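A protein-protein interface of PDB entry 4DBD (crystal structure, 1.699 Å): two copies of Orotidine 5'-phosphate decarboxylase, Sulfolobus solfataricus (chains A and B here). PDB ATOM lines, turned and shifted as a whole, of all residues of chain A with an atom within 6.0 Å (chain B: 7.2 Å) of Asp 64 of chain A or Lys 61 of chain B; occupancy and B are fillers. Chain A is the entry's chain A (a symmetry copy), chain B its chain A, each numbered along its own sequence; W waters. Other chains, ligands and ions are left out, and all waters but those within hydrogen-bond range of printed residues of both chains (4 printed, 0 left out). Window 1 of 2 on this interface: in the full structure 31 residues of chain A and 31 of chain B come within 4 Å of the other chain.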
ATOM      1  N   PHE A  60      20.848  26.455  -7.242  1.00  0.00           N
ATOM      2  CA  PHE A  60      20.800  25.191  -6.539  1.00  0.00           C
ATOM      3  C   PHE A  60      20.304  25.432  -5.109  1.00  0.00           C
ATOM      4  O   PHE A  60      20.507  24.585  -4.225  1.00  0.00           O
ATOM      5  CB  PHE A  60      22.191  24.552  -6.484  1.00  0.00           C
ATOM      6  CG  PHE A  60      22.694  24.055  -7.812  1.00  0.00           C
ATOM      7  CD1 PHE A  60      21.939  24.194  -8.969  1.00  0.00           C
ATOM      8  CD2 PHE A  60      23.928  23.435  -7.896  1.00  0.00           C
ATOM      9  CE1 PHE A  60      22.412  23.730 -10.183  1.00  0.00           C
ATOM     10  CE2 PHE A  60      24.406  22.965  -9.107  1.00  0.00           C
ATOM     11  CZ  PHE A  60      23.642  23.112 -10.254  1.00  0.00           C
ATOM     12  N   LYS A  61      19.668  26.588  -4.890  1.00  0.00           N
ATOM     13  CA  LYS A  61      19.115  26.945  -3.582  1.00  0.00           C
ATOM     14  C   LYS A  61      20.111  26.632  -2.481  1.00  0.00           C
ATOM     15  O   LYS A  61      19.788  25.941  -1.503  1.00  0.00           O
ATOM     16  CB  LYS A  61      17.811  26.200  -3.320  1.00  0.00           C
ATOM     17  CG  LYS A  61      16.623  26.644  -4.190  1.00  0.00           C
ATOM     18  CD  LYS A  61      16.282  28.118  -3.969  1.00  0.00           C
ATOM     19  CE  LYS A  61      14.888  28.455  -4.527  1.00  0.00           C
ATOM     20  NZ  LYS A  61      14.757  28.208  -6.007  1.00  0.00           N
ATOM     21  N   LEU A  62      21.315  27.167  -2.629  1.00  0.00           N
ATOM     22  CA  LEU A  62      22.441  26.797  -1.780  1.00  0.00           C
ATOM     23  C   LEU A  62      22.103  26.953  -0.301  1.00  0.00           C
ATOM     24  O   LEU A  62      21.602  27.988   0.129  1.00  0.00           O
ATOM     25  CB  LEU A  62      23.661  27.624  -2.147  1.00  0.00           C
ATOM     26  CG  LEU A  62      24.226  27.382  -3.558  1.00  0.00           C
ATOM     27  CD1 LEU A  62      25.137  28.528  -3.982  1.00  0.00           C
ATOM     28  CD2 LEU A  62      24.948  26.030  -3.642  1.00  0.00           C
ATOM     29  N   ALA A  63      22.367  25.911   0.482  1.00  0.00           N
ATOM     30  CA  ALA A  63      21.946  25.943   1.886  1.00  0.00           C
ATOM     31  C   ALA A  63      22.787  24.990   2.725  1.00  0.00           C
ATOM     32  O   ALA A  63      22.291  24.018   3.291  1.00  0.00           O
ATOM     33  CB  ALA A  63      20.475  25.622   1.996  1.00  0.00           C
ATOM     34  N   ASP A  64      24.079  25.264   2.780  1.00  0.00           N
ATOM     35  CA  ASP A  64      24.974  24.407   3.542  1.00  0.00           C
ATOM     36  C   ASP A  64      26.027  25.267   4.213  1.00  0.00           C
ATOM     37  O   ASP A  64      25.962  26.500   4.163  1.00  0.00           O
ATOM     38  CB  ASP A  64      25.606  23.355   2.615  1.00  0.00           C
ATOM     39  CG  ASP A  64      25.833  22.023   3.309  1.00  0.00           C
ATOM     40  OD1 ASP A  64      26.266  22.037   4.481  1.00  0.00           O
ATOM     41  OD2 ASP A  64      25.588  20.960   2.691  1.00  0.00           O
ATOM     42  N   ILE A  65      26.979  24.623   4.875  1.00  0.00           N
ATOM     43  CA  ILE A  65      28.112  25.338   5.429  1.00  0.00           C
ATOM     44  C   ILE A  65      28.967  25.901   4.289  1.00  0.00           C
ATOM     45  O   ILE A  65      28.865  25.455   3.132  1.00  0.00           O
ATOM     46  CB  ILE A  65      28.958  24.425   6.326  1.00  0.00           C
ATOM     47  CG1 ILE A  65      29.564  23.289   5.495  1.00  0.00           C
ATOM     48  CG2 ILE A  65      28.107  23.855   7.444  1.00  0.00           C
ATOM     49  CD1 ILE A  65      30.626  22.490   6.257  1.00  0.00           C
ATOM     50  N   GLY A  66      29.821  26.862   4.627  1.00  0.00           N
ATOM     51  CA  GLY A  66      30.578  27.611   3.640  1.00  0.00           C
ATOM     52  C   GLY A  66      31.450  26.722   2.792  1.00  0.00           C
ATOM     53  O   GLY A  66      31.459  26.856   1.565  1.00  0.00           O
ATOM     54  N   ILE A  68      31.139  23.713   1.889  1.00  0.00           N
ATOM     55  CA  ILE A  68      30.382  22.925   0.918  1.00  0.00           C
ATOM     56  C   ILE A  68      29.818  23.821  -0.176  1.00  0.00           C
ATOM     57  O   ILE A  68      29.842  23.462  -1.349  1.00  0.00           O
ATOM     58  CB  ILE A  68      29.232  22.153   1.590  1.00  0.00           C
ATOM     59  CG1 ILE A  68      29.771  21.087   2.557  1.00  0.00           C
ATOM     60  CG2 ILE A  68      28.307  21.558   0.549  1.00  0.00           C
ATOM     61  CD1 ILE A  68      30.577  19.996   1.908  1.00  0.00           C
ATOM     62  N   MET A  69      29.284  24.984   0.203  1.00  0.00           N
ATOM     63  CA  MET A  69      28.749  25.886  -0.806  1.00  0.00           C
ATOM     64  C   MET A  69      29.821  26.359  -1.771  1.00  0.00           C
ATOM     65  O   MET A  69      29.581  26.472  -2.967  1.00  0.00           O
ATOM     66  CB  MET A  69      28.028  27.061  -0.162  1.00  0.00           C
ATOM     67  CG  MET A  69      26.712  26.617   0.436  1.00  0.00           C
ATOM     68  SD  MET A  69      25.644  27.949   1.032  1.00  0.00           S
ATOM     69  CE  MET A  69      26.731  28.786   2.170  1.00  0.00           C
ATOM     70  N   ILE A  72      30.693  23.631  -4.230  1.00  0.00           N
ATOM     71  CA  ILE A  72      29.685  23.559  -5.269  1.00  0.00           C
ATOM     72  C   ILE A  72      29.899  24.618  -6.342  1.00  0.00           C
ATOM     73  O   ILE A  72      29.979  24.294  -7.533  1.00  0.00           O
ATOM     74  CB  ILE A  72      28.280  23.708  -4.663  1.00  0.00           C
ATOM     75  CG1 ILE A  72      27.967  22.502  -3.777  1.00  0.00           C
ATOM     76  CG2 ILE A  72      27.231  23.864  -5.755  1.00  0.00           C
ATOM     77  CD1 ILE A  72      26.722  22.664  -2.912  1.00  0.00           C
ATOM     78  N   ILE A  88      19.969  30.070   6.170  1.00  0.00           N
ATOM     79  CA  ILE A  88      21.148  29.360   6.692  1.00  0.00           C
ATOM     80  C   ILE A  88      22.066  30.237   7.539  1.00  0.00           C
ATOM     81  O   ILE A  88      22.893  29.727   8.296  1.00  0.00           O
ATOM     82  CB  ILE A  88      21.967  28.701   5.578  1.00  0.00           C
ATOM     83  CG1 ILE A  88      22.523  29.752   4.625  1.00  0.00           C
ATOM     84  CG2 ILE A  88      21.106  27.686   4.814  1.00  0.00           C
ATOM     85  CD1 ILE A  88      23.156  29.129   3.391  1.00  0.00           C
ATOM     86  N   GLY A  92      30.098  31.222   9.088  1.00  0.00           N
ATOM     87  CA  GLY A  92      30.462  29.861   8.726  1.00  0.00           C
ATOM     88  C   GLY A  92      29.614  29.308   7.589  1.00  0.00           C
ATOM     89  O   GLY A  92      29.690  28.121   7.262  1.00  0.00           O
ATOM     90  N   SER A  93      28.802  30.169   6.991  1.00  0.00           N
ATOM     91  CA  SER A  93      27.965  29.770   5.859  1.00  0.00           C
ATOM     92  C   SER A  93      27.978  30.876   4.806  1.00  0.00           C
ATOM     93  O   SER A  93      28.860  30.912   3.952  1.00  0.00           O
ATOM     94  CB  SER A  93      26.553  29.432   6.335  1.00  0.00           C
ATOM     95  OG  SER A  93      25.710  29.037   5.266  1.00  0.00           O
ATOM     96  N   LEU A  94      27.033  31.809   4.871  1.00  0.00           N
ATOM     97  CA  LEU A  94      26.990  32.838   3.837  1.00  0.00           C
ATOM     98  C   LEU A  94      28.197  33.788   3.813  1.00  0.00           C
ATOM     99  O   LEU A  94      28.571  34.281   2.742  1.00  0.00           O
ATOM    100  CB  LEU A  94      25.672  33.613   3.882  1.00  0.00           C
ATOM    101  CG  LEU A  94      24.450  32.795   3.459  1.00  0.00           C
ATOM    102  CD1 LEU A  94      23.183  33.549   3.821  1.00  0.00           C
ATOM    103  CD2 LEU A  94      24.486  32.471   1.948  1.00  0.00           C
ATOM    104  N   ASP B  11      32.249  13.992  -0.289  1.00  0.00           N
ATOM    105  CA  ASP B  11      32.194  15.274  -0.978  1.00  0.00           C
ATOM    106  C   ASP B  11      33.439  15.463  -1.849  1.00  0.00           C
ATOM    107  O   ASP B  11      33.584  16.474  -2.541  1.00  0.00           O
ATOM    108  CB  ASP B  11      32.076  16.402   0.051  1.00  0.00           C
ATOM    109  CG  ASP B  11      30.781  16.341   0.830  1.00  0.00           C
ATOM    110  OD1 ASP B  11      29.710  16.166   0.196  1.00  0.00           O
ATOM    111  OD2 ASP B  11      30.832  16.462   2.076  1.00  0.00           O
ATOM    112  N   LYS B  30      27.042   9.251   2.284  1.00  0.00           N
ATOM    113  CA  LYS B  30      26.236  10.428   1.972  1.00  0.00           C
ATOM    114  C   LYS B  30      26.872  11.160   0.790  1.00  0.00           C
ATOM    115  O   LYS B  30      27.990  11.673   0.878  1.00  0.00           O
ATOM    116  CB  LYS B  30      26.113  11.357   3.189  1.00  0.00           C
ATOM    117  CG  LYS B  30      25.169  12.547   2.976  1.00  0.00           C
ATOM    118  CD  LYS B  30      25.055  13.424   4.224  1.00  0.00           C
ATOM    119  CE  LYS B  30      26.268  14.322   4.421  1.00  0.00           C
ATOM    120  NZ  LYS B  30      26.337  15.432   3.438  1.00  0.00           N
ATOM    121  N   LEU B  33      26.476  17.405  -3.566  1.00  0.00           N
ATOM    122  CA  LEU B  33      26.635  18.117  -4.833  1.00  0.00           C
ATOM    123  C   LEU B  33      28.098  18.259  -5.265  1.00  0.00           C
ATOM    124  O   LEU B  33      28.404  18.195  -6.463  1.00  0.00           O
ATOM    125  CB  LEU B  33      25.971  19.493  -4.771  1.00  0.00           C
ATOM    126  CG  LEU B  33      24.548  19.548  -5.324  1.00  0.00           C
ATOM    127  CD1 LEU B  33      23.835  20.808  -4.852  1.00  0.00           C
ATOM    128  CD2 LEU B  33      24.572  19.456  -6.852  1.00  0.00           C
ATOM    129  N   PRO B  34      29.019  18.454  -4.301  1.00  0.00           N
ATOM    130  CA  PRO B  34      30.410  18.583  -4.752  1.00  0.00           C
ATOM    131  C   PRO B  34      30.882  17.365  -5.544  1.00  0.00           C
ATOM    132  O   PRO B  34      31.633  17.524  -6.523  1.00  0.00           O
ATOM    133  CB  PRO B  34      31.184  18.688  -3.444  1.00  0.00           C
ATOM    134  CG  PRO B  34      30.190  19.329  -2.485  1.00  0.00           C
ATOM    135  CD  PRO B  34      28.874  18.711  -2.853  1.00  0.00           C
ATOM    136  N   VAL B  58      21.449  10.733  -0.499  1.00  0.00           N
ATOM    137  CA  VAL B  58      21.804  11.864  -1.334  1.00  0.00           C
ATOM    138  C   VAL B  58      21.476  13.122  -0.532  1.00  0.00           C
ATOM    139  O   VAL B  58      20.357  13.275  -0.028  1.00  0.00           O
ATOM    140  CB  VAL B  58      21.050  11.856  -2.684  1.00  0.00           C
ATOM    141  CG1 VAL B  58      21.128  13.232  -3.317  1.00  0.00           C
ATOM    142  CG2 VAL B  58      21.655  10.799  -3.610  1.00  0.00           C
ATOM    143  N   ASP B  59      22.477  13.988  -0.384  1.00  0.00           N
ATOM    144  CA  ASP B  59      22.312  15.234   0.361  1.00  0.00           C
ATOM    145  C   ASP B  59      22.594  16.426  -0.555  1.00  0.00           C
ATOM    146  O   ASP B  59      23.735  16.868  -0.696  1.00  0.00           O
ATOM    147  CB  ASP B  59      23.221  15.260   1.602  1.00  0.00           C
ATOM    148  CG  ASP B  59      23.043  16.508   2.409  1.00  0.00           C
ATOM    149  OD1 ASP B  59      22.051  17.226   2.140  1.00  0.00           O
ATOM    150  OD2 ASP B  59      23.864  16.774   3.315  1.00  0.00           O
ATOM    151  N   PHE B  60      21.538  16.924  -1.192  1.00  0.00           N
ATOM    152  CA  PHE B  60      21.601  18.170  -1.926  1.00  0.00           C
ATOM    153  C   PHE B  60      20.902  19.265  -1.114  1.00  0.00           C
ATOM    154  O   PHE B  60      20.522  20.309  -1.667  1.00  0.00           O
ATOM    155  CB  PHE B  60      20.905  18.032  -3.282  1.00  0.00           C
ATOM    156  CG  PHE B  60      21.634  17.153  -4.262  1.00  0.00           C
ATOM    157  CD1 PHE B  60      22.826  16.527  -3.924  1.00  0.00           C
ATOM    158  CD2 PHE B  60      21.123  16.965  -5.535  1.00  0.00           C
ATOM    159  CE1 PHE B  60      23.487  15.723  -4.836  1.00  0.00           C
ATOM    160  CE2 PHE B  60      21.782  16.165  -6.453  1.00  0.00           C
ATOM    161  CZ  PHE B  60      22.970  15.544  -6.101  1.00  0.00           C
ATOM    162  N   LYS B  61      20.726  19.016   0.189  1.00  0.00           N
ATOM    163  CA  LYS B  61      20.097  19.980   1.095  1.00  0.00           C
ATOM    164  C   LYS B  61      18.852  20.571   0.461  1.00  0.00           C
ATOM    165  O   LYS B  61      18.695  21.798   0.384  1.00  0.00           O
ATOM    166  CB  LYS B  61      21.067  21.098   1.459  1.00  0.00           C
ATOM    167  CG  LYS B  61      22.236  20.674   2.364  1.00  0.00           C
ATOM    168  CD  LYS B  61      21.743  20.132   3.706  1.00  0.00           C
ATOM    169  CE  LYS B  61      22.885  20.077   4.736  1.00  0.00           C
ATOM    170  NZ  LYS B  61      24.030  19.191   4.317  1.00  0.00           N
ATOM    171  N   LEU B  62      17.955  19.693   0.034  1.00  0.00           N
ATOM    172  CA  LEU B  62      16.811  20.084  -0.781  1.00  0.00           C
ATOM    173  C   LEU B  62      16.008  21.201  -0.124  1.00  0.00           C
ATOM    174  O   LEU B  62      15.654  21.121   1.049  1.00  0.00           O
ATOM    175  CB  LEU B  62      15.932  18.875  -1.055  1.00  0.00           C
ATOM    176  CG  LEU B  62      16.576  17.767  -1.908  1.00  0.00           C
ATOM    177  CD1 LEU B  62      15.812  16.456  -1.760  1.00  0.00           C
ATOM    178  CD2 LEU B  62      16.683  18.191  -3.379  1.00  0.00           C
ATOM    179  N   ALA B  63      15.731  22.258  -0.880  1.00  0.00           N
ATOM    180  CA  ALA B  63      15.080  23.424  -0.276  1.00  0.00           C
ATOM    181  C   ALA B  63      14.355  24.248  -1.332  1.00  0.00           C
ATOM    182  O   ALA B  63      14.687  25.403  -1.591  1.00  0.00           O
ATOM    183  CB  ALA B  63      16.093  24.256   0.472  1.00  0.00           C
ATOM    184  N   ASP B  64      13.369  23.631  -1.962  1.00  0.00           N
ATOM    185  CA  ASP B  64      12.622  24.323  -3.000  1.00  0.00           C
ATOM    186  C   ASP B  64      11.164  23.916  -2.912  1.00  0.00           C
ATOM    187  O   ASP B  64      10.761  23.206  -1.985  1.00  0.00           O
ATOM    188  CB  ASP B  64      13.220  24.001  -4.378  1.00  0.00           C
ATOM    189  CG  ASP B  64      13.137  25.171  -5.342  1.00  0.00           C
ATOM    190  OD1 ASP B  64      12.087  25.848  -5.357  1.00  0.00           O
ATOM    191  OD2 ASP B  64      14.112  25.420  -6.091  1.00  0.00           O
ATOM    192  N   MET B  69      11.757  19.898  -6.117  1.00  0.00           N
ATOM    193  CA  MET B  69      12.412  18.860  -5.334  1.00  0.00           C
ATOM    194  C   MET B  69      12.157  17.475  -5.899  1.00  0.00           C
ATOM    195  O   MET B  69      13.048  16.634  -5.923  1.00  0.00           O
ATOM    196  CB  MET B  69      12.008  18.942  -3.870  1.00  0.00           C
ATOM    197  CG  MET B  69      12.650  20.140  -3.205  1.00  0.00           C
ATOM    198  SD  MET B  69      12.443  20.232  -1.411  1.00  0.00           S
ATOM    199  CE  MET B  69      10.669  20.164  -1.260  1.00  0.00           C
ATOM    200  N   PHE B  82      17.094  10.629   1.123  1.00  0.00           N
ATOM    201  CA  PHE B  82      17.353  11.990   0.681  1.00  0.00           C
ATOM    202  C   PHE B  82      17.245  12.961   1.849  1.00  0.00           C
ATOM    203  O   PHE B  82      16.363  12.834   2.688  1.00  0.00           O
ATOM    204  CB  PHE B  82      16.343  12.402  -0.396  1.00  0.00           C
ATOM    205  CG  PHE B  82      16.505  11.661  -1.685  1.00  0.00           C
ATOM    206  CD1 PHE B  82      17.420  12.089  -2.630  1.00  0.00           C
ATOM    207  CD2 PHE B  82      15.763  10.520  -1.931  1.00  0.00           C
ATOM    208  CE1 PHE B  82      17.578  11.395  -3.820  1.00  0.00           C
ATOM    209  CE2 PHE B  82      15.918   9.814  -3.114  1.00  0.00           C
ATOM    210  CZ  PHE B  82      16.820  10.249  -4.056  1.00  0.00           C
ATOM    211  N   ILE B  83      18.154  13.929   1.893  1.00  0.00           N
ATOM    212  CA  ILE B  83      18.125  14.971   2.915  1.00  0.00           C
ATOM    213  C   ILE B  83      17.489  16.243   2.343  1.00  0.00           C
ATOM    214  O   ILE B  83      17.844  16.703   1.249  1.00  0.00           O
ATOM    215  CB  ILE B  83      19.540  15.233   3.465  1.00  0.00           C
ATOM    216  CG1 ILE B  83      20.013  13.995   4.247  1.00  0.00           C
ATOM    217  CG2 ILE B  83      19.570  16.510   4.317  1.00  0.00           C
ATOM    218  CD1 ILE B  83      21.436  14.076   4.744  1.00  0.00           C
ATOM    219  N   ALA B  84      16.499  16.764   3.061  1.00  0.00           N
ATOM    220  CA  ALA B  84      15.886  18.053   2.736  1.00  0.00           C
ATOM    221  C   ALA B  84      15.888  18.943   3.963  1.00  0.00           C
ATOM    222  O   ALA B  84      15.965  18.452   5.088  1.00  0.00           O
ATOM    223  CB  ALA B  84      14.454  17.860   2.246  1.00  0.00           C
ATOM    224  N   HIS B  85      15.792  20.253   3.748  1.00  0.00           N
ATOM    225  CA  HIS B  85      15.704  21.203   4.864  1.00  0.00           C
ATOM    226  C   HIS B  85      14.301  21.270   5.431  1.00  0.00           C
ATOM    227  O   HIS B  85      13.338  21.322   4.682  1.00  0.00           O
ATOM    228  CB  HIS B  85      16.118  22.602   4.411  1.00  0.00           C
ATOM    229  CG  HIS B  85      17.577  22.880   4.571  1.00  0.00           C
ATOM    230  ND1 HIS B  85      18.165  23.082   5.801  1.00  0.00           N
ATOM    231  CD2 HIS B  85      18.568  22.981   3.653  1.00  0.00           C
ATOM    232  CE1 HIS B  85      19.459  23.294   5.636  1.00  0.00           C
ATOM    233  NE2 HIS B  85      19.729  23.238   4.343  1.00  0.00           N
ATOM    234  N   PHE B  87      13.270  23.896   7.146  1.00  0.00           N
ATOM    235  CA  PHE B  87      12.835  25.301   7.207  1.00  0.00           C
ATOM    236  C   PHE B  87      11.952  25.735   6.035  1.00  0.00           C
ATOM    237  O   PHE B  87      11.223  26.734   6.130  1.00  0.00           O
ATOM    238  CB  PHE B  87      14.020  26.268   7.408  1.00  0.00           C
ATOM    239  CG  PHE B  87      14.842  26.514   6.167  1.00  0.00           C
ATOM    240  CD1 PHE B  87      14.452  27.466   5.233  1.00  0.00           C
ATOM    241  CD2 PHE B  87      16.024  25.824   5.958  1.00  0.00           C
ATOM    242  CE1 PHE B  87      15.219  27.697   4.092  1.00  0.00           C
ATOM    243  CE2 PHE B  87      16.790  26.051   4.830  1.00  0.00           C
ATOM    244  CZ  PHE B  87      16.388  26.988   3.896  1.00  0.00           C
ATOM    245  N   ILE B  88      11.983  24.968   4.951  1.00  0.00           N
ATOM    246  CA  ILE B  88      11.148  25.292   3.782  1.00  0.00           C
ATOM    247  C   ILE B  88       9.658  25.055   4.008  1.00  0.00           C
ATOM    248  O   ILE B  88       8.823  25.573   3.265  1.00  0.00           O
ATOM    249  CB  ILE B  88      11.594  24.537   2.525  1.00  0.00           C
ATOM    250  CG1 ILE B  88      11.443  23.034   2.719  1.00  0.00           C
ATOM    251  CG2 ILE B  88      13.046  24.891   2.180  1.00  0.00           C
ATOM    252  CD1 ILE B  88      12.075  22.244   1.583  1.00  0.00           C
ATOM    253  N   VAL B 111      16.673  18.308   7.803  1.00  0.00           N
ATOM    254  CA  VAL B 111      17.688  19.063   8.527  1.00  0.00           C
ATOM    255  C   VAL B 111      17.056  19.864   9.666  1.00  0.00           C
ATOM    256  O   VAL B 111      16.196  20.723   9.433  1.00  0.00           O
ATOM    257  CB  VAL B 111      18.444  20.009   7.584  1.00  0.00           C
ATOM    258  CG1 VAL B 111      19.398  20.893   8.393  1.00  0.00           C
ATOM    259  CG2 VAL B 111      19.198  19.200   6.547  1.00  0.00           C
ATOM    260  N   MET B 114      21.942  22.832  12.136  1.00  0.00           N
ATOM    261  CA  MET B 114      23.267  22.748  11.515  1.00  0.00           C
ATOM    262  C   MET B 114      24.392  23.110  12.476  1.00  0.00           C
ATOM    263  O   MET B 114      24.151  23.652  13.561  1.00  0.00           O
ATOM    264  CB  MET B 114      23.333  23.566  10.233  1.00  0.00           C
ATOM    265  CG  MET B 114      22.272  23.146   9.242  1.00  0.00           C
ATOM    266  SD  MET B 114      22.611  23.737   7.582  1.00  0.00           S
ATOM    267  CE  MET B 114      24.203  22.953   7.281  1.00  0.00           C
ATOM    268  N   HIS B 116      27.261  25.081  11.937  1.00  0.00           N
ATOM    269  CA  HIS B 116      27.969  26.357  11.879  1.00  0.00           C
ATOM    270  C   HIS B 116      27.355  27.365  12.852  1.00  0.00           C
ATOM    271  O   HIS B 116      26.178  27.266  13.220  1.00  0.00           O
ATOM    272  CB  HIS B 116      27.997  26.908  10.450  1.00  0.00           C
ATOM    273  CG  HIS B 116      26.638  27.148   9.879  1.00  0.00           C
ATOM    274  ND1 HIS B 116      25.791  26.121   9.532  1.00  0.00           N
ATOM    275  CD2 HIS B 116      25.973  28.299   9.616  1.00  0.00           C
ATOM    276  CE1 HIS B 116      24.658  26.627   9.076  1.00  0.00           C
ATOM    277  NE2 HIS B 116      24.743  27.943   9.114  1.00  0.00           N
ATOM    278  N   VAL B 140      18.603  15.447  10.716  1.00  0.00           N
ATOM    279  CA  VAL B 140      20.009  15.790  10.789  1.00  0.00           C
ATOM    280  C   VAL B 140      20.180  16.801  11.919  1.00  0.00           C
ATOM    281  O   VAL B 140      19.599  17.879  11.869  1.00  0.00           O
ATOM    282  CB  VAL B 140      20.489  16.416   9.448  1.00  0.00           C
ATOM    283  CG1 VAL B 140      21.988  16.709   9.488  1.00  0.00           C
ATOM    284  CG2 VAL B 140      20.154  15.509   8.278  1.00  0.00           C
ATOM    285  N   PRO B 164      26.370  15.374  11.506  1.00  0.00           N
ATOM    286  CA  PRO B 164      27.603  15.766  10.823  1.00  0.00           C
ATOM    287  C   PRO B 164      28.387  16.715  11.708  1.00  0.00           C
ATOM    288  O   PRO B 164      28.001  16.928  12.854  1.00  0.00           O
ATOM    289  CB  PRO B 164      27.091  16.481   9.566  1.00  0.00           C
ATOM    290  CG  PRO B 164      25.757  17.038   9.961  1.00  0.00           C
ATOM    291  CD  PRO B 164      25.210  16.184  11.087  1.00  0.00           C
ATOM    292  N   GLN B 169      34.984  20.152  11.631  1.00  0.00           N
ATOM    293  CA  GLN B 169      34.113  21.223  12.114  1.00  0.00           C
ATOM    294  C   GLN B 169      34.089  21.331  13.636  1.00  0.00           C
ATOM    295  O   GLN B 169      33.442  22.231  14.182  1.00  0.00           O
ATOM    296  CB  GLN B 169      32.685  21.045  11.593  1.00  0.00           C
ATOM    297  CG  GLN B 169      32.542  21.172  10.087  1.00  0.00           C
ATOM    298  CD  GLN B 169      31.112  20.976   9.628  1.00  0.00           C
ATOM    299  OE1 GLN B 169      30.219  21.746   9.995  1.00  0.00           O
ATOM    300  NE2 GLN B 169      30.885  19.933   8.825  1.00  0.00           N
HETATM  301  O   HOH W   1      19.461  21.836  -3.870  1.00  0.00           O
HETATM  302  O   HOH W   2      22.040  22.530  -2.908  1.00  0.00           O
HETATM  303  O   HOH W   3      13.925  26.384  -8.763  1.00  0.00           O
HETATM  304  O   HOH W   4      27.074  18.544   2.927  1.00  0.00           O
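Of the 14 printed residues of chain A, 9 touch a printed residue of chain B.
Hydrophobic or aromatic side chains of chain A within 4 Å of the printed part of chain B: Ala 63, Ile 65, Ile 68 and Ile 72.
Hydrophobic or aromatic side chains of chain B that line the printed part of chain A: Leu 33, His 85, Met 114 and His 116.
The side-chain carboxylate of Asp 64 of chain A is in salt-bridge range of the side-chain amino group of Lys 61 of chain B, 2.9 Å away.
The side-chain amino group of Lys 61 of chain A lies within salt-bridge range of the side-chain carboxylate of Asp 64 of chain B (2.9 Å).
A ring nitrogen (NE2) of His 85 of chain B sits at hydrogen-bond distance from the backbone carbonyl oxygen (O) of Ala 63 of chain A (2.9 Å).
A ring nitrogen (NE2) of His 116 of chain B is in hydrogen-bond range of the backbone carbonyl oxygen of Ile 88 of chain A (2.7 Å).
Asp 64 of chain A touches just these residues of chain B: Lys 61 and Met 114.
Lys 61 of chain B touches just these residues of chain A: Ala 63 (3.5 Å) and Asp 64 (2.9 Å).
Of the printed residues of chain A, Asp 64 of chain B touches Lys 61 (2.9 Å).
Of the printed residues of chain A, Leu 33 of chain B touches Ile 72.
Of the printed residues of chain B, Ile 65 of chain A touches His 116 and Gln 169.
Val 140 of chain B touches none of the printed residues of chain A.
The nearest residue of chain A that does not touch Lys 61 of chain B is Lys 61 of chain A (4.7 Å).
The nearest printed residue of chain B that does not touch Ile 65 of chain A is Met 114 of chain B (4.01 Å).
Water W3 bridges the side-chain carboxylate (OD2) of Asp 64 of chain B (2.8 Å) and the side-chain amino group (NZ) of Lys 61 of chain A (3.4 Å).
Water W4 lies within hydrogen-bond range of OD2 of Asp 64 of chain A (2.8 Å), NZ of Lys 30 of chain B (3.2 Å) and NZ of Lys 61 of chain B (3.4 Å).
Water W1 bridges O of Phe 60 of chain B and O of Phe 60 of chain A.
Water W2 bridges O of Phe 60 of chain A (2.9 Å) and O of Phe 60 of chain B (3.0 Å).
O of Ala 63 of chain B touches CG of Lys 61 of chain A, 3.5 Å away.
O of Ala 63 of chain A touches CG of Lys 61 of chain B (3.5 Å).
Asp 64 of chain A touches Met 114 of chain B.
His 116 of chain B touches Ile 65 of chain A.
CD1 of Ile 65 of chain A touches NE2 of Gln 169 of chain B, 3.6 Å away.
CD1 of Ile 68 of chain A touches OD2 of Asp 11 of chain B, 3.5 Å away.
Ile 72 of chain A touches Leu 33 of chain B.
Gly 92 of chain A touches His 116 of chain B.
His 116 of chain B touches Ser 93 of chain A.
The side-chain carboxylate (OD2) of Asp 59 of chain B lies within salt-bridge range of the side-chain amino group (NZ) of Lys 61 of chain B.
The backbone carbonyl oxygen (O) of Leu 62 of chain B sits at hydrogen-bond distance from the backbone NH (N) of His 85 of chain B, at 2.8 Å.
N of Asp 64 of chain B lies within hydrogen-bond range of SD of Met 69 of chain B (3.6 Å).
SD of Met 69 of chain A is in hydrogen-bond range of N of Asp 64 of chain A, 3.6 Å away.
N of Gly 66 of chain A is in hydrogen-bond range of O of Gly 92 of chain A (2.9 Å).
Lys 61 of chain A touches Ala 63 of chain B, and with the chains exchanged Ala 63 of chain A touches Lys 61 of chain B.
Lys 61 of chain A touches Asp 64 of chain B, and with the chains exchanged Asp 64 of chain A touches Lys 61 of chain B.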
